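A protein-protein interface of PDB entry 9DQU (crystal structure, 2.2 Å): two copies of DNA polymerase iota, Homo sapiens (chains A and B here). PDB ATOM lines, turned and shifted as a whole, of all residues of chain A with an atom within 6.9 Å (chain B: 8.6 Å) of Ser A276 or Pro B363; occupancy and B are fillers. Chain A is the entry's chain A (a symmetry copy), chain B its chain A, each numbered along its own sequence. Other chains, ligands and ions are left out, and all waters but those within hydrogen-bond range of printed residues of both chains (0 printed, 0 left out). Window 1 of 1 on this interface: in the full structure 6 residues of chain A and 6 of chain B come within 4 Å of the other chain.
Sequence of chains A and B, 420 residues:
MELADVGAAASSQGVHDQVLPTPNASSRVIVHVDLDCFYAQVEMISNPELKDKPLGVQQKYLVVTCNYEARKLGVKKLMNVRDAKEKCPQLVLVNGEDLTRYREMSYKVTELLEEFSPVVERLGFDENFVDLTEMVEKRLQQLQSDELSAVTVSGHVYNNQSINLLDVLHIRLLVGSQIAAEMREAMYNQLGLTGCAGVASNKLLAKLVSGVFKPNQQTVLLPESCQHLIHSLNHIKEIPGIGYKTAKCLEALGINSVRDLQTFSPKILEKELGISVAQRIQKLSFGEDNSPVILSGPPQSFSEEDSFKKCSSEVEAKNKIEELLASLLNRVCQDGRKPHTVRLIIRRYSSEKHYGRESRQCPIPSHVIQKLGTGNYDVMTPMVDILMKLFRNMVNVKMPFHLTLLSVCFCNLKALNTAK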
ATOM      1  N   GLU A 270      14.144   8.718  15.723  1.00  0.00           N
ATOM      2  CA  GLU A 270      15.026   9.859  15.502  1.00  0.00           C
ATOM      3  C   GLU A 270      15.336  10.567  16.817  1.00  0.00           C
ATOM      4  O   GLU A 270      16.502  10.725  17.194  1.00  0.00           O
ATOM      5  CB  GLU A 270      14.392  10.837  14.512  1.00  0.00           C
ATOM      6  CG  GLU A 270      14.390  10.366  13.070  1.00  0.00           C
ATOM      7  CD  GLU A 270      13.389  11.124  12.217  1.00  0.00           C
ATOM      8  OE1 GLU A 270      12.492  11.776  12.791  1.00  0.00           O
ATOM      9  OE2 GLU A 270      13.499  11.069  10.974  1.00  0.00           O
ATOM     10  N   LEU A 273      17.649   8.536  19.112  1.00  0.00           N
ATOM     11  CA  LEU A 273      18.960   8.087  18.648  1.00  0.00           C
ATOM     12  C   LEU A 273      19.656   9.054  17.712  1.00  0.00           C
ATOM     13  O   LEU A 273      20.864   8.900  17.496  1.00  0.00           O
ATOM     14  CB  LEU A 273      18.850   6.739  17.930  1.00  0.00           C
ATOM     15  CG  LEU A 273      18.305   5.542  18.701  1.00  0.00           C
ATOM     16  CD1 LEU A 273      18.186   4.371  17.743  1.00  0.00           C
ATOM     17  CD2 LEU A 273      19.188   5.192  19.880  1.00  0.00           C
ATOM     18  N   GLY A 274      18.966  10.018  17.136  1.00  0.00           N
ATOM     19  CA  GLY A 274      19.559  10.866  16.132  1.00  0.00           C
ATOM     20  C   GLY A 274      19.032  10.534  14.748  1.00  0.00           C
ATOM     21  O   GLY A 274      18.635   9.398  14.457  1.00  0.00           O
ATOM     22  N   ILE A 275      19.054  11.534  13.875  1.00  0.00           N
ATOM     23  CA  ILE A 275      18.419  11.406  12.571  1.00  0.00           C
ATOM     24  C   ILE A 275      19.291  10.562  11.647  1.00  0.00           C
ATOM     25  O   ILE A 275      18.777   9.862  10.765  1.00  0.00           O
ATOM     26  CB  ILE A 275      18.145  12.807  11.997  1.00  0.00           C
ATOM     27  CG1 ILE A 275      17.392  13.702  13.006  1.00  0.00           C
ATOM     28  CG2 ILE A 275      17.328  12.711  10.717  1.00  0.00           C
ATOM     29  CD1 ILE A 275      18.212  14.269  14.195  1.00  0.00           C
ATOM     30  N   SER A 276      20.608  10.605  11.845  1.00  0.00           N
ATOM     31  CA  SER A 276      21.516   9.758  11.082  1.00  0.00           C
ATOM     32  C   SER A 276      21.329   8.288  11.437  1.00  0.00           C
ATOM     33  O   SER A 276      21.126   7.445  10.555  1.00  0.00           O
ATOM     34  CB  SER A 276      22.957  10.191  11.349  1.00  0.00           C
ATOM     35  OG  SER A 276      23.279  10.021  12.720  1.00  0.00           O
ATOM     36  N   VAL A 277      21.392   7.965  12.730  1.00  0.00           N
ATOM     37  CA  VAL A 277      21.380   6.570  13.162  1.00  0.00           C
ATOM     38  C   VAL A 277      20.010   5.947  12.912  1.00  0.00           C
ATOM     39  O   VAL A 277      19.893   4.914  12.243  1.00  0.00           O
ATOM     40  CB  VAL A 277      21.792   6.472  14.643  1.00  0.00           C
ATOM     41  CG1 VAL A 277      21.325   5.167  15.274  1.00  0.00           C
ATOM     42  CG2 VAL A 277      23.303   6.615  14.771  1.00  0.00           C
ATOM     43  N   ALA A 278      18.960   6.570  13.451  1.00  0.00           N
ATOM     44  CA  ALA A 278      17.604   6.057  13.265  1.00  0.00           C
ATOM     45  C   ALA A 278      17.320   5.747  11.801  1.00  0.00           C
ATOM     46  O   ALA A 278      16.845   4.658  11.463  1.00  0.00           O
ATOM     47  CB  ALA A 278      16.587   7.067  13.797  1.00  0.00           C
ATOM     48  N   GLN A 279      17.615   6.694  10.914  1.00  0.00           N
ATOM     49  CA  GLN A 279      17.241   6.528   9.515  1.00  0.00           C
ATOM     50  C   GLN A 279      17.988   5.367   8.870  1.00  0.00           C
ATOM     51  O   GLN A 279      17.395   4.575   8.128  1.00  0.00           O
ATOM     52  CB  GLN A 279      17.503   7.828   8.755  1.00  0.00           C
ATOM     53  CG  GLN A 279      16.930   7.853   7.347  1.00  0.00           C
ATOM     54  CD  GLN A 279      16.008   9.037   7.096  1.00  0.00           C
ATOM     55  OE1 GLN A 279      15.688   9.802   8.007  1.00  0.00           O
ATOM     56  NE2 GLN A 279      15.574   9.186   5.849  1.00  0.00           N
ATOM     57  N   ARG A 280      19.286   5.240   9.143  1.00  0.00           N
ATOM     58  CA  ARG A 280      20.078   4.206   8.484  1.00  0.00           C
ATOM     59  C   ARG A 280      19.756   2.821   9.037  1.00  0.00           C
ATOM     60  O   ARG A 280      19.561   1.872   8.270  1.00  0.00           O
ATOM     61  CB  ARG A 280      21.568   4.514   8.635  1.00  0.00           C
ATOM     62  CG  ARG A 280      22.514   3.487   8.013  1.00  0.00           C
ATOM     63  CD  ARG A 280      23.907   3.614   8.637  1.00  0.00           C
ATOM     64  NE  ARG A 280      24.101   4.948   9.197  1.00  0.00           N
ATOM     65  CZ  ARG A 280      24.358   5.214  10.473  1.00  0.00           C
ATOM     66  NH1 ARG A 280      24.559   4.251  11.360  1.00  0.00           N
ATOM     67  NH2 ARG A 280      24.407   6.483  10.873  1.00  0.00           N
ATOM     68  N   ILE A 281      19.707   2.676  10.363  1.00  0.00           N
ATOM     69  CA  ILE A 281      19.466   1.345  10.910  1.00  0.00           C
ATOM     70  C   ILE A 281      18.060   0.869  10.564  1.00  0.00           C
ATOM     71  O   ILE A 281      17.844  -0.328  10.345  1.00  0.00           O
ATOM     72  CB  ILE A 281      19.718   1.292  12.430  1.00  0.00           C
ATOM     73  CG1 ILE A 281      18.596   1.969  13.221  1.00  0.00           C
ATOM     74  CG2 ILE A 281      21.070   1.895  12.768  1.00  0.00           C
ATOM     75  CD1 ILE A 281      18.728   1.760  14.730  1.00  0.00           C
ATOM     76  N   LYS A 283      16.572   1.589   7.785  1.00  0.00           N
ATOM     77  CA  LYS A 283      16.784   1.105   6.424  1.00  0.00           C
ATOM     78  C   LYS A 283      17.422  -0.280   6.442  1.00  0.00           C
ATOM     79  O   LYS A 283      16.984  -1.186   5.726  1.00  0.00           O
ATOM     80  CB  LYS A 283      17.652   2.090   5.637  1.00  0.00           C
ATOM     81  CG  LYS A 283      16.855   3.094   4.806  1.00  0.00           C
ATOM     82  CD  LYS A 283      17.756   4.091   4.078  1.00  0.00           C
ATOM     83  CE  LYS A 283      18.038   5.332   4.921  1.00  0.00           C
ATOM     84  NZ  LYS A 283      19.475   5.747   4.869  1.00  0.00           N
ATOM     85  N   PRO B 339      26.740  18.220  -1.553  1.00  0.00           N
ATOM     86  CA  PRO B 339      27.159  18.011  -0.166  1.00  0.00           C
ATOM     87  C   PRO B 339      26.562  16.745   0.422  1.00  0.00           C
ATOM     88  O   PRO B 339      25.486  16.291   0.032  1.00  0.00           O
ATOM     89  CB  PRO B 339      26.625  19.257   0.551  1.00  0.00           C
ATOM     90  CG  PRO B 339      25.414  19.648  -0.257  1.00  0.00           C
ATOM     91  CD  PRO B 339      25.744  19.305  -1.679  1.00  0.00           C
ATOM     92  N   HIS B 340      27.283  16.177   1.390  1.00  0.00           N
ATOM     93  CA  HIS B 340      26.850  14.960   2.058  1.00  0.00           C
ATOM     94  C   HIS B 340      26.685  15.133   3.560  1.00  0.00           C
ATOM     95  O   HIS B 340      26.332  14.165   4.246  1.00  0.00           O
ATOM     96  CB  HIS B 340      27.836  13.822   1.773  1.00  0.00           C
ATOM     97  CG  HIS B 340      27.775  13.318   0.364  1.00  0.00           C
ATOM     98  ND1 HIS B 340      27.914  14.148  -0.727  1.00  0.00           N
ATOM     99  CD2 HIS B 340      27.576  12.075  -0.132  1.00  0.00           C
ATOM    100  CE1 HIS B 340      27.807  13.437  -1.836  1.00  0.00           C
ATOM    101  NE2 HIS B 340      27.604  12.175  -1.502  1.00  0.00           N
ATOM    102  N   THR B 341      26.917  16.330   4.090  1.00  0.00           N
ATOM    103  CA  THR B 341      26.704  16.608   5.501  1.00  0.00           C
ATOM    104  C   THR B 341      26.110  17.999   5.638  1.00  0.00           C
ATOM    105  O   THR B 341      26.484  18.915   4.900  1.00  0.00           O
ATOM    106  CB  THR B 341      28.009  16.517   6.302  1.00  0.00           C
ATOM    107  OG1 THR B 341      28.658  15.270   6.022  1.00  0.00           O
ATOM    108  CG2 THR B 341      27.727  16.625   7.799  1.00  0.00           C
ATOM    109  N   VAL B 342      25.172  18.146   6.570  1.00  0.00           N
ATOM    110  CA  VAL B 342      24.595  19.438   6.903  1.00  0.00           C
ATOM    111  C   VAL B 342      24.758  19.651   8.398  1.00  0.00           C
ATOM    112  O   VAL B 342      24.712  18.705   9.191  1.00  0.00           O
ATOM    113  CB  VAL B 342      23.107  19.554   6.502  1.00  0.00           C
ATOM    114  CG1 VAL B 342      22.219  18.794   7.482  1.00  0.00           C
ATOM    115  CG2 VAL B 342      22.692  21.019   6.444  1.00  0.00           C
ATOM    116  N   ARG B 343      24.955  20.906   8.780  1.00  0.00           N
ATOM    117  CA  ARG B 343      25.135  21.284  10.171  1.00  0.00           C
ATOM    118  C   ARG B 343      24.271  22.492  10.476  1.00  0.00           C
ATOM    119  O   ARG B 343      24.117  23.385   9.638  1.00  0.00           O
ATOM    120  CB  ARG B 343      26.596  21.612  10.469  1.00  0.00           C
ATOM    121  CG  ARG B 343      26.904  21.879  11.938  1.00  0.00           C
ATOM    122  CD  ARG B 343      28.412  21.793  12.163  1.00  0.00           C
ATOM    123  NE  ARG B 343      29.108  22.296  10.985  1.00  0.00           N
ATOM    124  CZ  ARG B 343      30.088  21.671  10.345  1.00  0.00           C
ATOM    125  NH1 ARG B 343      30.627  20.558  10.818  1.00  0.00           N
ATOM    126  NH2 ARG B 343      30.534  22.172   9.195  1.00  0.00           N
ATOM    127  N   ARG B 360      24.700  20.899  15.682  1.00  0.00           N
ATOM    128  CA  ARG B 360      24.378  19.513  15.384  1.00  0.00           C
ATOM    129  C   ARG B 360      24.498  19.324  13.881  1.00  0.00           C
ATOM    130  O   ARG B 360      24.015  20.160  13.114  1.00  0.00           O
ATOM    131  CB  ARG B 360      22.965  19.136  15.840  1.00  0.00           C
ATOM    132  CG  ARG B 360      22.712  19.306  17.322  1.00  0.00           C
ATOM    133  CD  ARG B 360      23.344  18.188  18.123  1.00  0.00           C
ATOM    134  NE  ARG B 360      23.060  18.330  19.545  1.00  0.00           N
ATOM    135  CZ  ARG B 360      23.800  19.031  20.395  1.00  0.00           C
ATOM    136  NH1 ARG B 360      24.897  19.657  20.005  1.00  0.00           N
ATOM    137  NH2 ARG B 360      23.426  19.107  21.670  1.00  0.00           N
ATOM    138  N   GLN B 361      25.145  18.245  13.464  1.00  0.00           N
ATOM    139  CA  GLN B 361      25.188  17.872  12.060  1.00  0.00           C
ATOM    140  C   GLN B 361      24.685  16.444  11.892  1.00  0.00           C
ATOM    141  O   GLN B 361      24.517  15.692  12.854  1.00  0.00           O
ATOM    142  CB  GLN B 361      26.603  17.999  11.491  1.00  0.00           C
ATOM    143  CG  GLN B 361      27.599  17.038  12.115  1.00  0.00           C
ATOM    144  CD  GLN B 361      29.036  17.397  11.793  1.00  0.00           C
ATOM    145  OE1 GLN B 361      29.582  18.364  12.326  1.00  0.00           O
ATOM    146  NE2 GLN B 361      29.657  16.615  10.917  1.00  0.00           N
ATOM    147  N   CYS B 362      24.457  16.081  10.641  1.00  0.00           N
ATOM    148  CA  CYS B 362      24.057  14.734  10.265  1.00  0.00           C
ATOM    149  C   CYS B 362      24.230  14.608   8.760  1.00  0.00           C
ATOM    150  O   CYS B 362      24.318  15.621   8.061  1.00  0.00           O
ATOM    151  CB  CYS B 362      22.602  14.448  10.672  1.00  0.00           C
ATOM    152  SG  CYS B 362      21.383  15.356   9.695  1.00  0.00           S
ATOM    153  N   PRO B 363      24.289  13.387   8.239  1.00  0.00           N
ATOM    154  CA  PRO B 363      24.427  13.223   6.792  1.00  0.00           C
ATOM    155  C   PRO B 363      23.150  13.633   6.078  1.00  0.00           C
ATOM    156  O   PRO B 363      22.073  13.742   6.671  1.00  0.00           O
ATOM    157  CB  PRO B 363      24.716  11.728   6.620  1.00  0.00           C
ATOM    158  CG  PRO B 363      24.988  11.207   8.013  1.00  0.00           C
ATOM    159  CD  PRO B 363      24.195  12.086   8.917  1.00  0.00           C
ATOM    160  N   ILE B 364      23.291  13.883   4.780  1.00  0.00           N
ATOM    161  CA  ILE B 364      22.192  14.326   3.934  1.00  0.00           C
ATOM    162  C   ILE B 364      21.648  13.087   3.204  1.00  0.00           C
ATOM    163  O   ILE B 364      22.326  12.585   2.298  1.00  0.00           O
ATOM    164  CB  ILE B 364      22.642  15.398   2.937  1.00  0.00           C
ATOM    165  CG1 ILE B 364      23.271  16.582   3.675  1.00  0.00           C
ATOM    166  CG2 ILE B 364      21.464  15.883   2.094  1.00  0.00           C
ATOM    167  CD1 ILE B 364      24.186  17.417   2.810  1.00  0.00           C
ATOM    168  N   PRO B 365      20.462  12.573   3.586  1.00  0.00           N
ATOM    169  CA  PRO B 365      19.907  11.395   2.897  1.00  0.00           C
ATOM    170  C   PRO B 365      20.203  11.348   1.408  1.00  0.00           C
ATOM    171  O   PRO B 365      20.030  12.346   0.703  1.00  0.00           O
ATOM    172  CB  PRO B 365      18.402  11.532   3.161  1.00  0.00           C
ATOM    173  CG  PRO B 365      18.312  12.242   4.489  1.00  0.00           C
ATOM    174  CD  PRO B 365      19.623  12.974   4.728  1.00  0.00           C
ATOM    175  N   SER B 366      20.665  10.191   0.924  1.00  0.00           N
ATOM    176  CA  SER B 366      21.009  10.072  -0.491  1.00  0.00           C
ATOM    177  C   SER B 366      19.805  10.380  -1.374  1.00  0.00           C
ATOM    178  O   SER B 366      19.951  10.946  -2.462  1.00  0.00           O
ATOM    179  CB  SER B 366      21.547   8.674  -0.787  1.00  0.00           C
ATOM    180  OG  SER B 366      22.243   8.656  -2.022  1.00  0.00           O
ATOM    181  N   VAL B 368      17.848  12.695  -0.963  1.00  0.00           N
ATOM    182  CA  VAL B 368      17.867  14.135  -1.183  1.00  0.00           C
ATOM    183  C   VAL B 368      19.006  14.527  -2.116  1.00  0.00           C
ATOM    184  O   VAL B 368      18.811  15.302  -3.059  1.00  0.00           O
ATOM    185  CB  VAL B 368      17.972  14.892   0.155  1.00  0.00           C
ATOM    186  CG1 VAL B 368      17.883  16.390  -0.096  1.00  0.00           C
ATOM    187  CG2 VAL B 368      16.895  14.442   1.122  1.00  0.00           C
ATOM    188  N   ILE B 369      20.212  14.000  -1.867  1.00  0.00           N
ATOM    189  CA  ILE B 369      21.400  14.444  -2.599  1.00  0.00           C
ATOM    190  C   ILE B 369      21.128  14.513  -4.096  1.00  0.00           C
ATOM    191  O   ILE B 369      21.767  15.291  -4.817  1.00  0.00           O
ATOM    192  CB  ILE B 369      22.598  13.518  -2.276  1.00  0.00           C
ATOM    193  CG1 ILE B 369      22.911  13.563  -0.774  1.00  0.00           C
ATOM    194  CG2 ILE B 369      23.844  13.916  -3.080  1.00  0.00           C
ATOM    195  CD1 ILE B 369      24.324  13.135  -0.413  1.00  0.00           C
ATOM    196  N   MET B 383      14.861  19.163   3.710  1.00  0.00           N
ATOM    197  CA  MET B 383      15.997  19.758   4.407  1.00  0.00           C
ATOM    198  C   MET B 383      15.547  20.487   5.668  1.00  0.00           C
ATOM    199  O   MET B 383      16.172  20.356   6.728  1.00  0.00           O
ATOM    200  CB  MET B 383      16.737  20.710   3.470  1.00  0.00           C
ATOM    201  CG  MET B 383      17.496  20.015   2.347  1.00  0.00           C
ATOM    202  SD  MET B 383      18.698  18.780   2.905  1.00  0.00           S
ATOM    203  CE  MET B 383      19.493  19.638   4.263  1.00  0.00           C
ATOM    204  N   ILE B 386      14.945  18.006   8.560  1.00  0.00           N
ATOM    205  CA  ILE B 386      16.187  17.582   9.204  1.00  0.00           C
ATOM    206  C   ILE B 386      16.673  18.662  10.161  1.00  0.00           C
ATOM    207  O   ILE B 386      16.950  18.404  11.339  1.00  0.00           O
ATOM    208  CB  ILE B 386      17.259  17.260   8.147  1.00  0.00           C
ATOM    209  CG1 ILE B 386      16.863  16.024   7.341  1.00  0.00           C
ATOM    210  CG2 ILE B 386      18.616  17.062   8.812  1.00  0.00           C
ATOM    211  CD1 ILE B 386      17.096  16.170   5.851  1.00  0.00           C
ATOM    212  N   LYS B 389      14.594  19.078  13.382  1.00  0.00           N
ATOM    213  CA  LYS B 389      14.975  18.021  14.313  1.00  0.00           C
ATOM    214  C   LYS B 389      16.306  18.359  14.973  1.00  0.00           C
ATOM    215  O   LYS B 389      16.422  18.370  16.205  1.00  0.00           O
ATOM    216  CB  LYS B 389      15.071  16.676  13.596  1.00  0.00           C
ATOM    217  CG  LYS B 389      13.773  16.172  12.987  1.00  0.00           C
ATOM    218  CD  LYS B 389      14.053  15.259  11.796  1.00  0.00           C
ATOM    219  CE  LYS B 389      12.874  15.184  10.845  1.00  0.00           C
ATOM    220  NZ  LYS B 389      12.259  13.828  10.835  1.00  0.00           N
ATOM    221  N   LEU B 390      17.326  18.641  14.155  1.00  0.00           N
ATOM    222  CA  LEU B 390      18.610  19.087  14.686  1.00  0.00           C
ATOM    223  C   LEU B 390      18.426  20.278  15.614  1.00  0.00           C
ATOM    224  O   LEU B 390      19.028  20.335  16.695  1.00  0.00           O
ATOM    225  CB  LEU B 390      19.558  19.445  13.538  1.00  0.00           C
ATOM    226  CG  LEU B 390      19.959  18.326  12.574  1.00  0.00           C
ATOM    227  CD1 LEU B 390      20.892  18.874  11.506  1.00  0.00           C
ATOM    228  CD2 LEU B 390      20.613  17.166  13.308  1.00  0.00           C
ATOM    229  N   CYS B 411      28.812  20.815   4.132  1.00  0.00           N
ATOM    230  CA  CYS B 411      30.189  20.386   3.929  1.00  0.00           C
ATOM    231  C   CYS B 411      30.181  18.964   3.385  1.00  0.00           C
ATOM    232  O   CYS B 411      29.119  18.382   3.132  1.00  0.00           O
ATOM    233  CB  CYS B 411      31.014  20.466   5.222  1.00  0.00           C
ATOM    234  SG  CYS B 411      30.199  19.839   6.698  1.00  0.00           S
ATOM    235  N   ASN B 412      31.378  18.411   3.181  1.00  0.00           N
ATOM    236  CA  ASN B 412      31.535  17.043   2.689  1.00  0.00           C
ATOM    237  C   ASN B 412      31.105  16.942   1.224  1.00  0.00           C
ATOM    238  O   ASN B 412      30.318  16.074   0.844  1.00  0.00           O
ATOM    239  CB  ASN B 412      30.749  16.067   3.565  1.00  0.00           C
ATOM    240  CG  ASN B 412      31.501  14.786   3.831  1.00  0.00           C
ATOM    241  OD1 ASN B 412      31.673  13.955   2.938  1.00  0.00           O
ATOM    242  ND2 ASN B 412      31.955  14.615   5.067  1.00  0.00           N
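Ser A276 touches just one residue of chain B: Pro B363 (3.3 Å).
Of chain A, only Ser A276 (3.3 Å) comes within 4 Å of Pro B363.
Printed residues of chain B within 4 Å of Ile A275: Lys B389 and Leu B390.
Of the printed residues of chain A, Leu B390 touches Ile A275 (3.9 Å).
Gln A279 touches none of the printed residues of chain B.
The nearest residue of chain B that does not touch Ser A276 is Cys B362 (4.3 Å).
The nearest residue of chain A that does not touch Pro B363 is Arg A280 (5.6 Å).
No position is printed for both chains.
Of the 4 pairs that touch across the chains among the printed residues, none has its exchanged pair printed and touching as well.
Among the printed residues, merely in contact across the chains: Ser A276 with Pro B363 (3.3 Å), Ile A275 with Lys B389 (3.8 Å) and Ile A275 with Leu B390 (3.9 Å).
O of Ser A276 lies within hydrogen-bond range of NH2 of Arg A280 (3.4 Å).
Of the 20 printed residues of chain B, 3 touch a printed residue of chain A.
Hydrophobic or aromatic side chains of chain B within 4 Å of the printed part of chain A: Pro B363 and Leu B390.
Among the printed residues, 4 pairs touch across the chains.
NZ of Lys B389 lies within salt-bridge range of OE1 of Glu A270 (2.8 Å).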
